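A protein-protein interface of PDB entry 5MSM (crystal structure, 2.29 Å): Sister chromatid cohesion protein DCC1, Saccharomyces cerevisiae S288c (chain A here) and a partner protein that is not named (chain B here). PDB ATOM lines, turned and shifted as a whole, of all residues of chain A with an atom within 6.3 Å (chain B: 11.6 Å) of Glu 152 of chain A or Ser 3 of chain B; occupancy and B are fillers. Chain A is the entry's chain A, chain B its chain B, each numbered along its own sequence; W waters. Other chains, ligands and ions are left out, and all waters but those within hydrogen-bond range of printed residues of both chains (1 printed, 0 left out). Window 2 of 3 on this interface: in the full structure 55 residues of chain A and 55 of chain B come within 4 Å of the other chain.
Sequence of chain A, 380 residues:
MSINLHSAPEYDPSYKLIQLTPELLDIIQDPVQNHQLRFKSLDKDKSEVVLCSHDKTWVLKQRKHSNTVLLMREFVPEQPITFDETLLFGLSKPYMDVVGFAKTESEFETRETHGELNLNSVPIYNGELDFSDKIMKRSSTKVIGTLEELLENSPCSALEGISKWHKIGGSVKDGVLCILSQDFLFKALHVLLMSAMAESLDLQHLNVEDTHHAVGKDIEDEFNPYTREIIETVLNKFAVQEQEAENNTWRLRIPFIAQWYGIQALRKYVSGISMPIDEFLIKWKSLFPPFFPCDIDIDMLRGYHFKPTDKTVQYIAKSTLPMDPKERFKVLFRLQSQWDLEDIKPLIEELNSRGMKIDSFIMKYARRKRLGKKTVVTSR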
ATOM      1  N   ARG A  38      -2.069 -30.908 -13.768  1.00  0.00           N
ATOM      2  CA  ARG A  38      -2.699 -29.924 -12.893  1.00  0.00           C
ATOM      3  C   ARG A  38      -2.405 -30.245 -11.427  1.00  0.00           C
ATOM      4  O   ARG A  38      -2.487 -31.403 -11.031  1.00  0.00           O
ATOM      5  CB  ARG A  38      -4.214 -29.897 -13.151  1.00  0.00           C
ATOM      6  CG  ARG A  38      -4.968 -28.742 -12.492  1.00  0.00           C
ATOM      7  CD  ARG A  38      -6.385 -28.528 -13.109  1.00  0.00           C
ATOM      8  NE  ARG A  38      -7.051 -27.297 -12.638  1.00  0.00           N
ATOM      9  CZ  ARG A  38      -6.765 -26.054 -13.042  1.00  0.00           C
ATOM     10  NH1 ARG A  38      -5.839 -25.844 -13.960  1.00  0.00           N
ATOM     11  NH2 ARG A  38      -7.423 -25.009 -12.552  1.00  0.00           N
ATOM     12  N   PHE A  39      -2.039 -29.234 -10.637  1.00  0.00           N
ATOM     13  CA  PHE A  39      -1.966 -29.381  -9.172  1.00  0.00           C
ATOM     14  C   PHE A  39      -3.326 -29.002  -8.576  1.00  0.00           C
ATOM     15  O   PHE A  39      -3.943 -28.036  -9.013  1.00  0.00           O
ATOM     16  CB  PHE A  39      -0.884 -28.481  -8.541  1.00  0.00           C
ATOM     17  CG  PHE A  39       0.537 -28.920  -8.801  1.00  0.00           C
ATOM     18  CD1 PHE A  39       1.062 -30.038  -8.191  1.00  0.00           C
ATOM     19  CD2 PHE A  39       1.354 -28.187  -9.646  1.00  0.00           C
ATOM     20  CE1 PHE A  39       2.377 -30.432  -8.436  1.00  0.00           C
ATOM     21  CE2 PHE A  39       2.666 -28.573  -9.891  1.00  0.00           C
ATOM     22  CZ  PHE A  39       3.178 -29.697  -9.283  1.00  0.00           C
ATOM     23  N   LYS A  40      -3.744 -29.693  -7.523  1.00  0.00           N
ATOM     24  CA  LYS A  40      -5.043 -29.425  -6.908  1.00  0.00           C
ATOM     25  C   LYS A  40      -4.949 -29.622  -5.415  1.00  0.00           C
ATOM     26  O   LYS A  40      -4.178 -30.463  -4.941  1.00  0.00           O
ATOM     27  CB  LYS A  40      -6.116 -30.371  -7.459  1.00  0.00           C
ATOM     28  CG  LYS A  40      -6.549 -30.073  -8.888  1.00  0.00           C
ATOM     29  CD  LYS A  40      -6.938 -31.348  -9.623  1.00  0.00           C
ATOM     30  CE  LYS A  40      -8.177 -31.971  -8.996  1.00  0.00           C
ATOM     31  NZ  LYS A  40      -9.297 -31.036  -9.116  1.00  0.00           N
ATOM     32  N   SER A  41      -5.740 -28.863  -4.668  1.00  0.00           N
ATOM     33  CA  SER A  41      -5.874 -29.138  -3.240  1.00  0.00           C
ATOM     34  C   SER A  41      -7.182 -28.566  -2.728  1.00  0.00           C
ATOM     35  O   SER A  41      -7.681 -27.576  -3.256  1.00  0.00           O
ATOM     36  CB  SER A  41      -4.670 -28.555  -2.462  1.00  0.00           C
ATOM     37  OG  SER A  41      -4.556 -29.085  -1.147  1.00  0.00           O
ATOM     38  N   LEU A  42      -7.724 -29.159  -1.678  1.00  0.00           N
ATOM     39  CA  LEU A  42      -8.958 -28.633  -1.105  1.00  0.00           C
ATOM     40  C   LEU A  42      -8.763 -27.235  -0.556  1.00  0.00           C
ATOM     41  O   LEU A  42      -9.633 -26.380  -0.681  1.00  0.00           O
ATOM     42  CB  LEU A  42      -9.467 -29.532   0.021  1.00  0.00           C
ATOM     43  CG  LEU A  42     -10.020 -30.909  -0.339  1.00  0.00           C
ATOM     44  CD1 LEU A  42     -11.203 -31.211   0.565  1.00  0.00           C
ATOM     45  CD2 LEU A  42     -10.394 -31.042  -1.814  1.00  0.00           C
ATOM     46  N   LEU A 147     -21.427 -31.595 -11.248  1.00  0.00           N
ATOM     47  CA  LEU A 147     -20.404 -32.607 -11.140  1.00  0.00           C
ATOM     48  C   LEU A 147     -19.024 -31.976 -11.312  1.00  0.00           C
ATOM     49  O   LEU A 147     -18.045 -32.419 -10.703  1.00  0.00           O
ATOM     50  CB  LEU A 147     -20.651 -33.682 -12.182  1.00  0.00           C
ATOM     51  CG  LEU A 147     -19.787 -34.927 -12.074  1.00  0.00           C
ATOM     52  CD1 LEU A 147     -19.947 -35.502 -10.677  1.00  0.00           C
ATOM     53  CD2 LEU A 147     -20.204 -35.919 -13.150  1.00  0.00           C
ATOM     54  N   GLU A 148     -18.965 -30.926 -12.132  1.00  0.00           N
ATOM     55  CA  GLU A 148     -17.723 -30.188 -12.365  1.00  0.00           C
ATOM     56  C   GLU A 148     -17.246 -29.537 -11.075  1.00  0.00           C
ATOM     57  O   GLU A 148     -16.062 -29.563 -10.755  1.00  0.00           O
ATOM     58  CB  GLU A 148     -17.920 -29.120 -13.439  1.00  0.00           C
ATOM     59  CG  GLU A 148     -18.383 -29.666 -14.790  1.00  0.00           C
ATOM     60  CD  GLU A 148     -19.895 -29.904 -14.828  1.00  0.00           C
ATOM     61  OE1 GLU A 148     -20.644 -28.910 -14.743  1.00  0.00           O
ATOM     62  OE2 GLU A 148     -20.333 -31.075 -14.927  1.00  0.00           O
ATOM     63  N   GLU A 149     -18.178 -28.951 -10.332  1.00  0.00           N
ATOM     64  CA  GLU A 149     -17.847 -28.358  -9.046  1.00  0.00           C
ATOM     65  C   GLU A 149     -17.373 -29.465  -8.102  1.00  0.00           C
ATOM     66  O   GLU A 149     -16.379 -29.300  -7.388  1.00  0.00           O
ATOM     67  CB  GLU A 149     -19.044 -27.607  -8.436  1.00  0.00           C
ATOM     68  CG  GLU A 149     -18.623 -26.566  -7.390  1.00  0.00           C
ATOM     69  CD  GLU A 149     -19.695 -26.232  -6.355  1.00  0.00           C
ATOM     70  OE1 GLU A 149     -20.916 -26.346  -6.668  1.00  0.00           O
ATOM     71  OE2 GLU A 149     -19.300 -25.851  -5.221  1.00  0.00           O
ATOM     72  N   LEU A 150     -18.099 -30.583  -8.082  1.00  0.00           N
ATOM     73  CA  LEU A 150     -17.691 -31.717  -7.264  1.00  0.00           C
ATOM     74  C   LEU A 150     -16.255 -32.123  -7.612  1.00  0.00           C
ATOM     75  O   LEU A 150     -15.412 -32.233  -6.729  1.00  0.00           O
ATOM     76  CB  LEU A 150     -18.632 -32.901  -7.462  1.00  0.00           C
ATOM     77  CG  LEU A 150     -18.415 -34.081  -6.517  1.00  0.00           C
ATOM     78  CD1 LEU A 150     -18.925 -33.687  -5.166  1.00  0.00           C
ATOM     79  CD2 LEU A 150     -19.130 -35.327  -6.972  1.00  0.00           C
ATOM     80  N   LEU A 151     -15.964 -32.284  -8.902  1.00  0.00           N
ATOM     81  CA  LEU A 151     -14.635 -32.730  -9.338  1.00  0.00           C
ATOM     82  C   LEU A 151     -13.567 -31.720  -8.973  1.00  0.00           C
ATOM     83  O   LEU A 151     -12.503 -32.094  -8.494  1.00  0.00           O
ATOM     84  CB  LEU A 151     -14.613 -32.977 -10.841  1.00  0.00           C
ATOM     85  CG  LEU A 151     -15.547 -34.107 -11.258  1.00  0.00           C
ATOM     86  CD1 LEU A 151     -15.448 -34.383 -12.751  1.00  0.00           C
ATOM     87  CD2 LEU A 151     -15.238 -35.343 -10.452  1.00  0.00           C
ATOM     88  N   GLU A 152     -13.869 -30.439  -9.174  1.00  0.00           N
ATOM     89  CA  GLU A 152     -12.920 -29.362  -8.890  1.00  0.00           C
ATOM     90  C   GLU A 152     -12.468 -29.357  -7.451  1.00  0.00           C
ATOM     91  O   GLU A 152     -11.324 -29.035  -7.155  1.00  0.00           O
ATOM     92  CB  GLU A 152     -13.557 -28.005  -9.215  1.00  0.00           C
ATOM     93  CG  GLU A 152     -12.656 -26.789  -8.998  1.00  0.00           C
ATOM     94  CD  GLU A 152     -11.283 -26.906  -9.652  1.00  0.00           C
ATOM     95  OE1 GLU A 152     -11.172 -27.539 -10.729  1.00  0.00           O
ATOM     96  OE2 GLU A 152     -10.311 -26.346  -9.086  1.00  0.00           O
ATOM     97  N   ASN A 153     -13.350 -29.786  -6.566  1.00  0.00           N
ATOM     98  CA  ASN A 153     -13.020 -29.870  -5.155  1.00  0.00           C
ATOM     99  C   ASN A 153     -12.679 -31.287  -4.696  1.00  0.00           C
ATOM    100  O   ASN A 153     -12.916 -31.643  -3.537  1.00  0.00           O
ATOM    101  CB  ASN A 153     -14.175 -29.317  -4.319  1.00  0.00           C
ATOM    102  CG  ASN A 153     -13.689 -28.414  -3.201  1.00  0.00           C
ATOM    103  OD1 ASN A 153     -12.632 -27.772  -3.318  1.00  0.00           O
ATOM    104  ND2 ASN A 153     -14.445 -28.369  -2.104  1.00  0.00           N
ATOM    105  N   SER A 154     -12.124 -32.088  -5.601  1.00  0.00           N
ATOM    106  CA  SER A 154     -11.821 -33.478  -5.300  1.00  0.00           C
ATOM    107  C   SER A 154     -10.364 -33.814  -5.541  1.00  0.00           C
ATOM    108  O   SER A 154      -9.735 -33.251  -6.439  1.00  0.00           O
ATOM    109  CB  SER A 154     -12.692 -34.411  -6.147  1.00  0.00           C
ATOM    110  OG  SER A 154     -13.989 -34.534  -5.611  1.00  0.00           O
ATOM    111  N   PRO B   2      -7.710 -24.970  -4.255  1.00  0.00           N
ATOM    112  CA  PRO B   2      -7.421 -24.384  -5.566  1.00  0.00           C
ATOM    113  C   PRO B   2      -6.809 -25.386  -6.532  1.00  0.00           C
ATOM    114  O   PRO B   2      -6.590 -26.558  -6.204  1.00  0.00           O
ATOM    115  CB  PRO B   2      -6.419 -23.280  -5.244  1.00  0.00           C
ATOM    116  CG  PRO B   2      -5.761 -23.738  -3.999  1.00  0.00           C
ATOM    117  CD  PRO B   2      -6.824 -24.438  -3.210  1.00  0.00           C
ATOM    118  N   SER B   3      -6.524 -24.903  -7.730  1.00  0.00           N
ATOM    119  CA  SER B   3      -5.974 -25.725  -8.780  1.00  0.00           C
ATOM    120  C   SER B   3      -5.218 -24.799  -9.692  1.00  0.00           C
ATOM    121  O   SER B   3      -5.487 -23.591  -9.716  1.00  0.00           O
ATOM    122  CB  SER B   3      -7.062 -26.451  -9.572  1.00  0.00           C
ATOM    123  OG  SER B   3      -8.159 -26.798  -8.761  1.00  0.00           O
ATOM    124  N   VAL B   4      -4.258 -25.358 -10.414  1.00  0.00           N
ATOM    125  CA  VAL B   4      -3.544 -24.628 -11.461  1.00  0.00           C
ATOM    126  C   VAL B   4      -2.839 -25.615 -12.374  1.00  0.00           C
ATOM    127  O   VAL B   4      -2.415 -26.685 -11.937  1.00  0.00           O
ATOM    128  CB  VAL B   4      -2.521 -23.633 -10.879  1.00  0.00           C
ATOM    129  CG1 VAL B   4      -1.479 -24.361 -10.041  1.00  0.00           C
ATOM    130  CG2 VAL B   4      -1.879 -22.801 -12.006  1.00  0.00           C
ATOM    131  N   ASP B   5      -2.736 -25.278 -13.651  1.00  0.00           N
ATOM    132  CA  ASP B   5      -2.024 -26.141 -14.588  1.00  0.00           C
ATOM    133  C   ASP B   5      -0.549 -25.820 -14.614  1.00  0.00           C
ATOM    134  O   ASP B   5      -0.135 -24.700 -14.329  1.00  0.00           O
ATOM    135  CB  ASP B   5      -2.583 -26.007 -16.003  1.00  0.00           C
ATOM    136  CG  ASP B   5      -4.027 -26.437 -16.101  1.00  0.00           C
ATOM    137  OD1 ASP B   5      -4.475 -27.294 -15.302  1.00  0.00           O
ATOM    138  OD2 ASP B   5      -4.730 -25.882 -16.966  1.00  0.00           O
ATOM    139  N   ILE B   6       0.235 -26.818 -14.985  1.00  0.00           N
ATOM    140  CA  ILE B   6       1.652 -26.645 -15.236  1.00  0.00           C
ATOM    141  C   ILE B   6       1.910 -26.196 -16.672  1.00  0.00           C
ATOM    142  O   ILE B   6       1.634 -26.925 -17.616  1.00  0.00           O
ATOM    143  CB  ILE B   6       2.384 -27.947 -14.966  1.00  0.00           C
ATOM    144  CG1 ILE B   6       2.242 -28.289 -13.483  1.00  0.00           C
ATOM    145  CG2 ILE B   6       3.876 -27.832 -15.371  1.00  0.00           C
ATOM    146  CD1 ILE B   6       2.666 -29.685 -13.148  1.00  0.00           C
ATOM    147  N   ASP B   7       2.457 -25.016 -16.828  1.00  0.00           N
ATOM    148  CA  ASP B   7       2.769 -24.507 -18.128  1.00  0.00           C
ATOM    149  C   ASP B   7       4.119 -25.018 -18.620  1.00  0.00           C
ATOM    150  O   ASP B   7       5.153 -24.697 -18.100  1.00  0.00           O
ATOM    151  CB  ASP B   7       2.754 -22.996 -18.109  1.00  0.00           C
ATOM    152  CG  ASP B   7       3.273 -22.402 -19.368  1.00  0.00           C
ATOM    153  OD1 ASP B   7       2.899 -22.850 -20.437  1.00  0.00           O
ATOM    154  OD2 ASP B   7       4.074 -21.487 -19.303  1.00  0.00           O
ATOM    155  N   PHE B 106       7.737 -21.905  -9.179  1.00  0.00           N
ATOM    156  CA  PHE B 106       6.434 -21.572  -8.594  1.00  0.00           C
ATOM    157  C   PHE B 106       6.295 -20.079  -8.355  1.00  0.00           C
ATOM    158  O   PHE B 106       6.820 -19.535  -7.375  1.00  0.00           O
ATOM    159  CB  PHE B 106       6.239 -22.360  -7.307  1.00  0.00           C
ATOM    160  CG  PHE B 106       6.058 -23.825  -7.546  1.00  0.00           C
ATOM    161  CD1 PHE B 106       7.155 -24.644  -7.784  1.00  0.00           C
ATOM    162  CD2 PHE B 106       4.789 -24.388  -7.579  1.00  0.00           C
ATOM    163  CE1 PHE B 106       6.994 -26.003  -8.030  1.00  0.00           C
ATOM    164  CE2 PHE B 106       4.624 -25.744  -7.817  1.00  0.00           C
ATOM    165  CZ  PHE B 106       5.733 -26.550  -8.052  1.00  0.00           C
ATOM    166  N   ASN B 107       5.559 -19.430  -9.249  1.00  0.00           N
ATOM    167  CA  ASN B 107       5.294 -18.005  -9.143  1.00  0.00           C
ATOM    168  C   ASN B 107       4.122 -17.725  -8.191  1.00  0.00           C
ATOM    169  O   ASN B 107       2.974 -17.907  -8.554  1.00  0.00           O
ATOM    170  CB  ASN B 107       5.022 -17.440 -10.533  1.00  0.00           C
ATOM    171  CG  ASN B 107       4.580 -15.995 -10.509  1.00  0.00           C
ATOM    172  OD1 ASN B 107       4.734 -15.293  -9.508  1.00  0.00           O
ATOM    173  ND2 ASN B 107       4.010 -15.539 -11.623  1.00  0.00           N
ATOM    174  N   SER B 108       4.443 -17.246  -6.988  1.00  0.00           N
ATOM    175  CA  SER B 108       3.497 -17.140  -5.889  1.00  0.00           C
ATOM    176  C   SER B 108       2.507 -16.031  -6.107  1.00  0.00           C
ATOM    177  O   SER B 108       1.395 -16.112  -5.615  1.00  0.00           O
ATOM    178  CB  SER B 108       4.217 -16.905  -4.551  1.00  0.00           C
ATOM    179  OG  SER B 108       4.731 -18.108  -3.985  1.00  0.00           O
ATOM    180  N   LYS B 109       2.925 -14.984  -6.809  1.00  0.00           N
ATOM    181  CA  LYS B 109       2.049 -13.847  -7.052  1.00  0.00           C
ATOM    182  C   LYS B 109       0.754 -14.318  -7.702  1.00  0.00           C
ATOM    183  O   LYS B 109      -0.352 -14.025  -7.211  1.00  0.00           O
ATOM    184  CB  LYS B 109       2.746 -12.829  -7.930  1.00  0.00           C
ATOM    185  CG  LYS B 109       1.902 -11.675  -8.397  1.00  0.00           C
ATOM    186  CD  LYS B 109       2.624 -10.967  -9.553  1.00  0.00           C
ATOM    187  CE  LYS B 109       1.711  -9.960 -10.218  1.00  0.00           C
ATOM    188  NZ  LYS B 109       2.490  -9.060 -11.089  1.00  0.00           N
ATOM    189  N   ASP B 110       0.909 -15.071  -8.787  1.00  0.00           N
ATOM    190  CA  ASP B 110      -0.214 -15.604  -9.547  1.00  0.00           C
ATOM    191  C   ASP B 110      -0.627 -17.026  -9.165  1.00  0.00           C
ATOM    192  O   ASP B 110      -1.624 -17.520  -9.690  1.00  0.00           O
ATOM    193  CB  ASP B 110       0.106 -15.585 -11.049  1.00  0.00           C
ATOM    194  CG  ASP B 110       0.431 -14.195 -11.566  1.00  0.00           C
ATOM    195  OD1 ASP B 110      -0.165 -13.214 -11.049  1.00  0.00           O
ATOM    196  OD2 ASP B 110       1.263 -14.088 -12.504  1.00  0.00           O
ATOM    197  N   ASN B 111       0.087 -17.663  -8.233  1.00  0.00           N
ATOM    198  CA  ASN B 111      -0.065 -19.108  -8.017  1.00  0.00           C
ATOM    199  C   ASN B 111      -0.025 -19.859  -9.351  1.00  0.00           C
ATOM    200  O   ASN B 111      -0.920 -20.645  -9.656  1.00  0.00           O
ATOM    201  CB  ASN B 111      -1.392 -19.431  -7.302  1.00  0.00           C
ATOM    202  CG  ASN B 111      -1.358 -19.146  -5.821  1.00  0.00           C
ATOM    203  OD1 ASN B 111      -0.395 -18.587  -5.287  1.00  0.00           O
ATOM    204  ND2 ASN B 111      -2.437 -19.505  -5.141  1.00  0.00           N
ATOM    205  N   LYS B 112       0.998 -19.598 -10.159  1.00  0.00           N
ATOM    206  CA  LYS B 112       1.177 -20.316 -11.413  1.00  0.00           C
ATOM    207  C   LYS B 112       2.537 -21.016 -11.436  1.00  0.00           C
ATOM    208  O   LYS B 112       3.459 -20.643 -10.703  1.00  0.00           O
ATOM    209  CB  LYS B 112       1.000 -19.361 -12.589  1.00  0.00           C
ATOM    210  CG  LYS B 112      -0.489 -19.157 -12.940  1.00  0.00           C
ATOM    211  CD  LYS B 112      -0.686 -18.084 -14.012  1.00  0.00           C
ATOM    212  CE  LYS B 112       0.639 -17.693 -14.662  1.00  0.00           C
ATOM    213  NZ  LYS B 112       0.646 -16.279 -15.138  1.00  0.00           N
ATOM    214  N   VAL B 113       2.642 -22.066 -12.241  1.00  0.00           N
ATOM    215  CA  VAL B 113       3.835 -22.885 -12.220  1.00  0.00           C
ATOM    216  C   VAL B 113       4.294 -23.274 -13.609  1.00  0.00           C
ATOM    217  O   VAL B 113       3.515 -23.710 -14.454  1.00  0.00           O
ATOM    218  CB  VAL B 113       3.627 -24.141 -11.355  1.00  0.00           C
ATOM    219  CG1 VAL B 113       2.328 -24.812 -11.694  1.00  0.00           C
ATOM    220  CG2 VAL B 113       4.821 -25.098 -11.484  1.00  0.00           C
HETATM  221  O   HOH W   1      -4.602 -23.245 -14.715  1.00  0.00           O
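The side-chain carboxylate (OD1) of Asp 5 of chain B is in salt-bridge range of the guanidinium group (NH1) of Arg 38 of chain A (2.4 Å). The backbone carbonyl oxygen (O) of Val 4 of chain B is in hydrogen-bond range of the backbone NH (N) of Phe 39 of chain A. The backbone NH of Ser 41 of chain A is in hydrogen-bond range of the backbone carbonyl oxygen of Pro 2 of chain B. The side-chain carboxylate (OE2) of Glu 152 of chain A lies close to the side-chain hydroxyl (OG) of Ser 3 of chain B (2.2 Å).
The side-chain amino group (NZ) of Lys 40 of chain A sits at hydrogen-bond distance from the backbone carbonyl oxygen (O) of Leu 151 of chain A (3.4 Å). The side-chain amino group of Lys 40 of chain A is in hydrogen-bond range of the backbone carbonyl oxygen of Glu 152 of chain A.
Ser 3 of chain B touches Arg 38 of chain A (CB to NE, 3.2 Å). CG of Arg 38 of chain A touches O of Val 4 of chain B (3.3 Å). O of Phe 39 of chain A touches CA of Ser 3 of chain B, at 3.1 Å. Phe 39 of chain A touches Ile 6 of chain B (CE2 to CD1, 3.4 Å). Pro 2 of chain B touches Lys 40 of chain A. Ser 3 of chain B touches Lys 40 of chain A (OG to CG, 3.7 Å).
Glu 152 of chain A touches just one residue of chain B: Ser 3. Printed residues of chain A within 4 Å of Ser 3 of chain B: Arg 38, Phe 39, Lys 40 and Glu 152. No residue of chain B comes within 4 Å of Leu 150 of chain A. No residue of chain B comes within 4 Å of Leu 151 of chain A. No residue of chain B comes within 4 Å of Asn 153 of chain A. Ser 154 of chain A touches none of the printed residues of chain B. Of the printed residues of chain B, Ser 41 of chain A touches Pro 2. Printed residues of chain B within 4 Å of Arg 38 of chain A: Ser 3 (3.2 Å), Val 4 (3.3 Å) and Asp 5 (2.4 Å). Of the printed residues of chain A, Ile 6 of chain B touches Phe 39 (3.4 Å). Of the printed residues of chain B, Phe 39 of chain A touches Ser 3 (3.1 Å), Val 4 (2.9 Å) and Ile 6 (3.4 Å). Asp 7 of chain B touches none of the printed residues of chain A. Asn 111 of chain B touches none of the printed residues of chain A. The nearest residue of chain B that does not touch Glu 152 of chain A is Pro 2 of chain B (4.4 Å). The nearest residue of chain A that does not touch Ser 3 of chain B is Ser 41 of chain A (5.1 Å).
Hydrophobic or aromatic side chains of chain B that line the printed part of chain A: Pro 2 and Ile 6. Along chain B the printed residues that touch a printed residue of chain A span positions 2 to 6. Hydrophobic or aromatic side chains of chain A within 4 Å of the printed part of chain B: Phe 39. Among the printed residues, 10 pairs touch across the chains. Among the printed residues, Asp or Glu carboxylates within 4 Å of a Lys or Arg side-chain nitrogen of the other chain: Arg 38 of chain A with Asp 5 of chain B (2.4 Å).
Water W1 bridges the backbone NH of Asp 5 of chain B and the guanidinium group of Arg 38 of chain A.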
